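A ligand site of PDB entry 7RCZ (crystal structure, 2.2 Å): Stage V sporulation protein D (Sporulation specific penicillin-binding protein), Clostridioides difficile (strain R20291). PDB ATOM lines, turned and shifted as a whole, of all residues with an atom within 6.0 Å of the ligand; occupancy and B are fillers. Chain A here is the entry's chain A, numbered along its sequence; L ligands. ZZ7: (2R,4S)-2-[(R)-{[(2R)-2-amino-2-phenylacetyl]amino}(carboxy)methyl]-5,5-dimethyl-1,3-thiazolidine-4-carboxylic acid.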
ATOM      1  N   PRO A 272       3.449 -11.361  35.278  1.00  0.00           N
ATOM      2  CA  PRO A 272       3.469 -12.766  34.881  1.00  0.00           C
ATOM      3  C   PRO A 272       4.485 -13.143  33.795  1.00  0.00           C
ATOM      4  O   PRO A 272       4.581 -14.294  33.529  1.00  0.00           O
ATOM      5  CB  PRO A 272       2.057 -13.015  34.331  1.00  0.00           C
ATOM      6  CG  PRO A 272       1.608 -11.659  33.835  1.00  0.00           C
ATOM      7  CD  PRO A 272       2.248 -10.667  34.773  1.00  0.00           C
ATOM      8  N   GLY A 273       5.124 -12.170  33.162  1.00  0.00           N
ATOM      9  CA  GLY A 273       6.066 -12.448  32.088  1.00  0.00           C
ATOM     10  C   GLY A 273       5.397 -12.999  30.837  1.00  0.00           C
ATOM     11  O   GLY A 273       4.220 -12.794  30.632  1.00  0.00           O
ATOM     12  N   SER A 274       6.126 -13.830  30.118  1.00  0.00           N
ATOM     13  CA  SER A 274       5.704 -14.379  28.804  1.00  0.00           C
ATOM     14  C   SER A 274       4.502 -15.344  28.861  1.00  0.00           C
ATOM     15  O   SER A 274       4.055 -15.697  27.826  1.00  0.00           O
ATOM     16  CB  SER A 274       6.878 -14.849  27.997  1.00  0.00           C
ATOM     17  OG  SER A 274       7.808 -13.809  27.810  1.00  0.00           O
ATOM     18  N   THR A 275       4.078 -15.825  30.025  1.00  0.00           N
ATOM     19  CA  THR A 275       2.831 -16.625  30.117  1.00  0.00           C
ATOM     20  C   THR A 275       1.674 -15.782  29.561  1.00  0.00           C
ATOM     21  O   THR A 275       0.820 -16.356  28.944  1.00  0.00           O
ATOM     22  CB  THR A 275       2.579 -17.170  31.536  1.00  0.00           C
ATOM     23  OG1 THR A 275       2.504 -16.048  32.388  1.00  0.00           O
ATOM     24  CG2 THR A 275       3.665 -18.101  32.025  1.00  0.00           C
ATOM     25  N   LYS A 277       1.707 -14.051  27.045  1.00  0.00           N
ATOM     26  CA  LYS A 277       1.711 -14.112  25.564  1.00  0.00           C
ATOM     27  C   LYS A 277       0.595 -15.041  25.074  1.00  0.00           C
ATOM     28  O   LYS A 277       0.183 -14.882  23.908  1.00  0.00           O
ATOM     29  CB  LYS A 277       3.064 -14.575  25.032  1.00  0.00           C
ATOM     30  CG  LYS A 277       4.198 -13.585  25.257  1.00  0.00           C
ATOM     31  CD  LYS A 277       5.460 -13.921  24.512  1.00  0.00           C
ATOM     32  CE  LYS A 277       6.550 -12.922  24.831  1.00  0.00           C
ATOM     33  NZ  LYS A 277       7.887 -13.405  24.413  1.00  0.00           N
ATOM     34  N   LYS A 310      13.990  -5.221  23.149  1.00  0.00           N
ATOM     35  CA  LYS A 310      14.852  -6.293  22.558  1.00  0.00           C
ATOM     36  C   LYS A 310      14.132  -7.645  22.661  1.00  0.00           C
ATOM     37  O   LYS A 310      13.487  -7.911  23.688  1.00  0.00           O
ATOM     38  CB  LYS A 310      16.188  -6.406  23.296  1.00  0.00           C
ATOM     39  CG  LYS A 310      17.113  -5.189  23.240  1.00  0.00           C
ATOM     40  CD  LYS A 310      18.163  -5.187  24.365  1.00  0.00           C
ATOM     41  CE  LYS A 310      19.121  -4.011  24.322  1.00  0.00           C
ATOM     42  NZ  LYS A 310      20.479  -4.413  23.861  1.00  0.00           N
ATOM     43  N   TRP A 312      14.737 -11.535  23.464  1.00  0.00           N
ATOM     44  CA  TRP A 312      15.670 -12.217  24.397  1.00  0.00           C
ATOM     45  C   TRP A 312      16.905 -12.695  23.622  1.00  0.00           C
ATOM     46  O   TRP A 312      17.989 -12.729  24.223  1.00  0.00           O
ATOM     47  CB  TRP A 312      14.953 -13.354  25.151  1.00  0.00           C
ATOM     48  CG  TRP A 312      14.753 -14.582  24.316  1.00  0.00           C
ATOM     49  CD1 TRP A 312      13.663 -14.883  23.559  1.00  0.00           C
ATOM     50  CD2 TRP A 312      15.701 -15.655  24.129  1.00  0.00           C
ATOM     51  NE1 TRP A 312      13.864 -16.072  22.904  1.00  0.00           N
ATOM     52  CE2 TRP A 312      15.096 -16.572  23.244  1.00  0.00           C
ATOM     53  CE3 TRP A 312      16.973 -15.933  24.641  1.00  0.00           C
ATOM     54  CZ2 TRP A 312      15.738 -17.746  22.853  1.00  0.00           C
ATOM     55  CZ3 TRP A 312      17.592 -17.102  24.255  1.00  0.00           C
ATOM     56  CH2 TRP A 312      16.981 -17.998  23.376  1.00  0.00           C
ATOM     57  N   ASN A 329       9.280 -19.376  20.002  1.00  0.00           N
ATOM     58  CA  ASN A 329      10.546 -18.615  20.136  1.00  0.00           C
ATOM     59  C   ASN A 329      10.458 -17.568  21.236  1.00  0.00           C
ATOM     60  O   ASN A 329      11.516 -16.986  21.586  1.00  0.00           O
ATOM     61  CB  ASN A 329      10.934 -17.932  18.827  1.00  0.00           C
ATOM     62  CG  ASN A 329      11.339 -18.925  17.757  1.00  0.00           C
ATOM     63  OD1 ASN A 329      11.807 -20.016  18.084  1.00  0.00           O
ATOM     64  ND2 ASN A 329      11.125 -18.593  16.498  1.00  0.00           N
ATOM     65  N   SER A 330       9.263 -17.307  21.759  1.00  0.00           N
ATOM     66  CA  SER A 330       8.967 -16.222  22.726  1.00  0.00           C
ATOM     67  C   SER A 330       9.568 -14.891  22.217  1.00  0.00           C
ATOM     68  O   SER A 330      10.202 -14.165  22.977  1.00  0.00           O
ATOM     69  CB  SER A 330       9.489 -16.601  24.094  1.00  0.00           C
ATOM     70  OG  SER A 330       8.785 -15.871  25.083  1.00  0.00           O
ATOM     71  N   ASN A 332       9.732 -11.354  21.520  1.00  0.00           N
ATOM     72  CA  ASN A 332       9.079 -10.121  22.043  1.00  0.00           C
ATOM     73  C   ASN A 332       8.613  -9.188  20.932  1.00  0.00           C
ATOM     74  O   ASN A 332       7.461  -8.763  20.958  1.00  0.00           O
ATOM     75  CB  ASN A 332       9.980  -9.382  23.039  1.00  0.00           C
ATOM     76  CG  ASN A 332      10.028 -10.087  24.360  1.00  0.00           C
ATOM     77  OD1 ASN A 332       9.294 -11.054  24.575  1.00  0.00           O
ATOM     78  ND2 ASN A 332      10.885  -9.618  25.254  1.00  0.00           N
ATOM     79  N   PHE A 388       3.770  -8.615  26.342  1.00  0.00           N
ATOM     80  CA  PHE A 388       4.589  -9.791  26.793  1.00  0.00           C
ATOM     81  C   PHE A 388       4.678  -9.809  28.323  1.00  0.00           C
ATOM     82  O   PHE A 388       5.664 -10.297  28.879  1.00  0.00           O
ATOM     83  CB  PHE A 388       5.937  -9.864  26.064  1.00  0.00           C
ATOM     84  CG  PHE A 388       6.839  -8.653  26.150  1.00  0.00           C
ATOM     85  CD1 PHE A 388       7.585  -8.383  27.289  1.00  0.00           C
ATOM     86  CD2 PHE A 388       6.955  -7.780  25.081  1.00  0.00           C
ATOM     87  CE1 PHE A 388       8.414  -7.277  27.373  1.00  0.00           C
ATOM     88  CE2 PHE A 388       7.782  -6.665  25.162  1.00  0.00           C
ATOM     89  CZ  PHE A 388       8.500  -6.411  26.311  1.00  0.00           C
ATOM     90  N   GLN A 390       4.690  -7.674  31.030  1.00  0.00           N
ATOM     91  CA  GLN A 390       5.373  -6.754  31.968  1.00  0.00           C
ATOM     92  C   GLN A 390       4.550  -5.462  32.031  1.00  0.00           C
ATOM     93  O   GLN A 390       3.839  -5.177  31.042  1.00  0.00           O
ATOM     94  CB  GLN A 390       6.838  -6.588  31.533  1.00  0.00           C
ATOM     95  CG  GLN A 390       7.822  -6.481  32.689  1.00  0.00           C
ATOM     96  CD  GLN A 390       8.000  -7.746  33.496  1.00  0.00           C
ATOM     97  OE1 GLN A 390       7.845  -8.847  32.974  1.00  0.00           O
ATOM     98  NE2 GLN A 390       8.344  -7.614  34.762  1.00  0.00           N
ATOM     99  N   GLY A 461      10.096 -23.373  23.565  1.00  0.00           N
ATOM    100  CA  GLY A 461      10.705 -23.020  24.863  1.00  0.00           C
ATOM    101  C   GLY A 461      10.208 -23.816  26.042  1.00  0.00           C
ATOM    102  O   GLY A 461      10.792 -23.623  27.139  1.00  0.00           O
ATOM    103  N   LYS A 475       3.483 -22.516  28.270  1.00  0.00           N
ATOM    104  CA  LYS A 475       4.299 -21.321  28.015  1.00  0.00           C
ATOM    105  C   LYS A 475       5.094 -21.011  29.269  1.00  0.00           C
ATOM    106  O   LYS A 475       4.520 -21.134  30.414  1.00  0.00           O
ATOM    107  CB  LYS A 475       3.394 -20.142  27.685  1.00  0.00           C
ATOM    108  CG  LYS A 475       4.109 -18.949  27.085  1.00  0.00           C
ATOM    109  CD  LYS A 475       4.646 -19.163  25.676  1.00  0.00           C
ATOM    110  CE  LYS A 475       5.647 -18.064  25.335  1.00  0.00           C
ATOM    111  NZ  LYS A 475       6.852 -18.139  26.211  1.00  0.00           N
ATOM    112  N   THR A 476       6.306 -20.544  29.068  1.00  0.00           N
ATOM    113  CA  THR A 476       7.235 -20.091  30.131  1.00  0.00           C
ATOM    114  C   THR A 476       7.205 -18.573  30.289  1.00  0.00           C
ATOM    115  O   THR A 476       6.898 -17.861  29.316  1.00  0.00           O
ATOM    116  CB  THR A 476       8.689 -20.475  29.816  1.00  0.00           C
ATOM    117  OG1 THR A 476       9.024 -20.025  28.490  1.00  0.00           O
ATOM    118  CG2 THR A 476       8.860 -21.978  29.873  1.00  0.00           C
ATOM    119  N   GLY A 477       7.543 -18.120  31.474  1.00  0.00           N
ATOM    120  CA  GLY A 477       7.890 -16.718  31.683  1.00  0.00           C
ATOM    121  C   GLY A 477       9.062 -16.567  32.614  1.00  0.00           C
ATOM    122  O   GLY A 477       9.186 -17.358  33.562  1.00  0.00           O
ATOM    123  N   THR A 478       9.836 -15.518  32.380  1.00  0.00           N
ATOM    124  CA  THR A 478      10.922 -14.993  33.239  1.00  0.00           C
ATOM    125  C   THR A 478      10.724 -13.467  33.266  1.00  0.00           C
ATOM    126  O   THR A 478      10.831 -12.873  32.196  1.00  0.00           O
ATOM    127  CB  THR A 478      12.283 -15.445  32.695  1.00  0.00           C
ATOM    128  OG1 THR A 478      12.156 -16.767  32.146  1.00  0.00           O
ATOM    129  CG2 THR A 478      13.360 -15.408  33.756  1.00  0.00           C
ATOM    130  N   ALA A 479      10.323 -12.917  34.397  1.00  0.00           N
ATOM    131  CA  ALA A 479      10.023 -11.489  34.591  1.00  0.00           C
ATOM    132  C   ALA A 479      10.871 -10.935  35.726  1.00  0.00           C
ATOM    133  O   ALA A 479      10.869 -11.563  36.798  1.00  0.00           O
ATOM    134  CB  ALA A 479       8.558 -11.309  34.910  1.00  0.00           C
ATOM    135  N   GLN A 480      11.548  -9.807  35.492  1.00  0.00           N
ATOM    136  CA  GLN A 480      12.248  -9.056  36.557  1.00  0.00           C
ATOM    137  C   GLN A 480      11.214  -8.713  37.615  1.00  0.00           C
ATOM    138  O   GLN A 480      10.047  -8.449  37.236  1.00  0.00           O
ATOM    139  CB  GLN A 480      12.924  -7.794  36.031  1.00  0.00           C
ATOM    140  CG  GLN A 480      13.935  -7.200  36.999  1.00  0.00           C
ATOM    141  CD  GLN A 480      15.063  -6.491  36.287  1.00  0.00           C
ATOM    142  OE1 GLN A 480      16.223  -6.876  36.378  1.00  0.00           O
ATOM    143  NE2 GLN A 480      14.707  -5.455  35.535  1.00  0.00           N
ATOM    144  N   TYR A 492      14.287 -12.182  39.948  1.00  0.00           N
ATOM    145  CA  TYR A 492      13.343 -12.626  38.902  1.00  0.00           C
ATOM    146  C   TYR A 492      12.221 -13.460  39.525  1.00  0.00           C
ATOM    147  O   TYR A 492      12.386 -14.032  40.634  1.00  0.00           O
ATOM    148  CB  TYR A 492      14.114 -13.370  37.813  1.00  0.00           C
ATOM    149  CG  TYR A 492      15.169 -12.537  37.129  1.00  0.00           C
ATOM    150  CD1 TYR A 492      14.880 -11.767  36.014  1.00  0.00           C
ATOM    151  CD2 TYR A 492      16.476 -12.504  37.609  1.00  0.00           C
ATOM    152  CE1 TYR A 492      15.846 -11.001  35.379  1.00  0.00           C
ATOM    153  CE2 TYR A 492      17.457 -11.753  36.979  1.00  0.00           C
ATOM    154  CZ  TYR A 492      17.137 -10.991  35.871  1.00  0.00           C
ATOM    155  OH  TYR A 492      18.105 -10.240  35.260  1.00  0.00           O
ATOM    156  N   ALA A 521      18.107 -18.765  36.233  1.00  0.00           N
ATOM    157  CA  ALA A 521      16.801 -18.144  36.559  1.00  0.00           C
ATOM    158  C   ALA A 521      15.936 -18.019  35.296  1.00  0.00           C
ATOM    159  O   ALA A 521      15.767 -16.924  34.800  1.00  0.00           O
ATOM    160  CB  ALA A 521      17.036 -16.813  37.247  1.00  0.00           C
ATOM    161  N   PHE A 522      15.368 -19.121  34.811  1.00  0.00           N
ATOM    162  CA  PHE A 522      14.449 -19.126  33.647  1.00  0.00           C
ATOM    163  C   PHE A 522      13.219 -19.934  34.011  1.00  0.00           C
ATOM    164  O   PHE A 522      13.294 -20.838  34.848  1.00  0.00           O
ATOM    165  CB  PHE A 522      15.110 -19.656  32.378  1.00  0.00           C
ATOM    166  CG  PHE A 522      16.291 -18.809  31.968  1.00  0.00           C
ATOM    167  CD1 PHE A 522      16.099 -17.640  31.269  1.00  0.00           C
ATOM    168  CD2 PHE A 522      17.574 -19.174  32.322  1.00  0.00           C
ATOM    169  CE1 PHE A 522      17.182 -16.846  30.936  1.00  0.00           C
ATOM    170  CE2 PHE A 522      18.657 -18.372  31.977  1.00  0.00           C
ATOM    171  CZ  PHE A 522      18.465 -17.208  31.300  1.00  0.00           C
ATOM    172  N   GLY A 523      12.091 -19.583  33.406  1.00  0.00           N
ATOM    173  CA  GLY A 523      10.815 -20.310  33.573  1.00  0.00           C
ATOM    174  C   GLY A 523      11.007 -21.775  33.215  1.00  0.00           C
ATOM    175  O   GLY A 523      10.594 -22.608  33.992  1.00  0.00           O
ATOM    176  N   SER A 524      11.650 -22.047  32.070  1.00  0.00           N
ATOM    177  CA  SER A 524      11.860 -23.409  31.531  1.00  0.00           C
ATOM    178  C   SER A 524      12.585 -24.267  32.557  1.00  0.00           C
ATOM    179  O   SER A 524      12.108 -25.334  32.811  1.00  0.00           O
ATOM    180  CB  SER A 524      12.551 -23.394  30.188  1.00  0.00           C
ATOM    181  OG  SER A 524      13.843 -22.845  30.293  1.00  0.00           O
HETATM  182  O1  ZZ7 L   1      11.774 -17.953  29.906  1.00  0.00           O
HETATM  183  C2  ZZ7 L   1      11.098 -17.428  28.991  1.00  0.00           C
HETATM  184  O2  ZZ7 L   1      10.256 -17.965  28.245  1.00  0.00           O
HETATM  185  C12 ZZ7 L   1      11.295 -15.925  28.622  1.00  0.00           C
HETATM  186  C6  ZZ7 L   1      12.664 -15.724  27.898  1.00  0.00           C
HETATM  187  C1  ZZ7 L   1      13.862 -15.568  28.863  1.00  0.00           C
HETATM  188  C16 ZZ7 L   1      12.932 -16.815  26.803  1.00  0.00           C
HETATM  189  S1  ZZ7 L   1      12.344 -14.066  26.986  1.00  0.00           S
HETATM  190  N3  ZZ7 L   1      10.142 -15.434  27.637  1.00  0.00           N
HETATM  191  C13 ZZ7 L   1      10.525 -14.106  27.011  1.00  0.00           C
HETATM  192  C14 ZZ7 L   1      10.000 -12.927  27.977  1.00  0.00           C
HETATM  193  C15 ZZ7 L   1       8.760 -13.568  28.658  1.00  0.00           C
HETATM  194  O4  ZZ7 L   1       8.818 -13.884  29.858  1.00  0.00           O
HETATM  195  N1  ZZ7 L   1      10.898 -12.453  29.072  1.00  0.00           N
HETATM  196  C3  ZZ7 L   1      11.709 -11.304  28.908  1.00  0.00           C
HETATM  197  O3  ZZ7 L   1      11.715 -10.753  27.819  1.00  0.00           O
HETATM  198  C4  ZZ7 L   1      12.654 -10.756  30.131  1.00  0.00           C
HETATM  199  N2  ZZ7 L   1      12.896  -9.257  30.058  1.00  0.00           N
HETATM  200  C5  ZZ7 L   1      13.991 -11.601  30.181  1.00  0.00           C
HETATM  201  C7  ZZ7 L   1      14.422 -12.245  31.387  1.00  0.00           C
HETATM  202  C8  ZZ7 L   1      15.613 -13.020  31.411  1.00  0.00           C
HETATM  203  C9  ZZ7 L   1      16.397 -13.155  30.223  1.00  0.00           C
HETATM  204  C10 ZZ7 L   1      15.997 -12.504  29.010  1.00  0.00           C
HETATM  205  C11 ZZ7 L   1      14.797 -11.740  28.997  1.00  0.00           C
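The backbone NH (N) of Ser 274 lies within hydrogen-bond range of an oxygen (O4) of the ligand (2.7 Å).
The side-chain amide nitrogen of Asn 332 sits at hydrogen-bond distance from an oxygen (O3) of the ligand (2.9 Å).
The backbone NH (N) of Thr 478 lies within hydrogen-bond range of an oxygen (O4) of the ligand.
The side-chain hydroxyl (OG) of Ser 330 is in hydrogen-bond range of a nitrogen (N3) of the ligand (2.9 Å).
A nitrogen (N1) of the ligand is in hydrogen-bond range of the backbone carbonyl oxygen (O) of Thr 478, 3.2 Å away.
The side-chain hydroxyl of Thr 478 lies within hydrogen-bond range of an oxygen (O1) of the ligand, 2.6 Å away.
An oxygen (O2) of the ligand lies within hydrogen-bond range of the side-chain hydroxyl (OG1) of Thr 476 (2.4 Å).
The side-chain hydroxyl (OG) of Ser 274 is covalently linked to a carbon (C15) of the ligand (1.3 Å).
The side-chain amino group of Lys 475 lies within salt-bridge range of an oxygen (O2) of the ligand (3.97 Å).
Gly 273 touches the ligand.
Lys 277 touches the ligand.
CB of Trp 312 touches S1 of the ligand (3.3 Å).
Gly 477 touches the ligand.
CE1 of Phe 522 touches C9 of the ligand, at 3.8 Å.
Gly 523 touches the ligand (N to O1, 3.9 Å).
Hydrophobic or aromatic side chains that line the ligand: Trp 312 and Phe 522.
Within 4 Å of the ligand: Gly 273, Ser 274, Lys 277, Trp 312, Ser 330, Asn 332, Lys 475, Thr 476, Gly 477, Thr 478, Phe 522 and Gly 523.
The backbone carbonyl oxygen (O) of Lys 310 is in hydrogen-bond range of the side-chain amide nitrogen (ND2) of Asn 332 (3.5 Å).
The side-chain hydroxyl (OG1) of Thr 478 is in hydrogen-bond range of the backbone NH (N) of Gly 523, 3.1 Å away.
The side-chain amino group of Lys 475 lies within hydrogen-bond range of the side-chain hydroxyl of Ser 330, 3.2 Å away.
The side-chain amino group (NZ) of Lys 277 is in hydrogen-bond range of the side-chain amide oxygen (OD1) of Asn 332 (2.7 Å).
The backbone carbonyl oxygen (O) of Asn 329 is in hydrogen-bond range of the indole nitrogen (NE1) of Trp 312 (2.8 Å).
The side-chain hydroxyl of Ser 330 is in hydrogen-bond range of the side-chain amino group of Lys 277, 2.7 Å away.
The side-chain hydroxyl (OG) of Ser 274 lies close to the side-chain amino group (NZ) of Lys 277 (3.4 Å).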
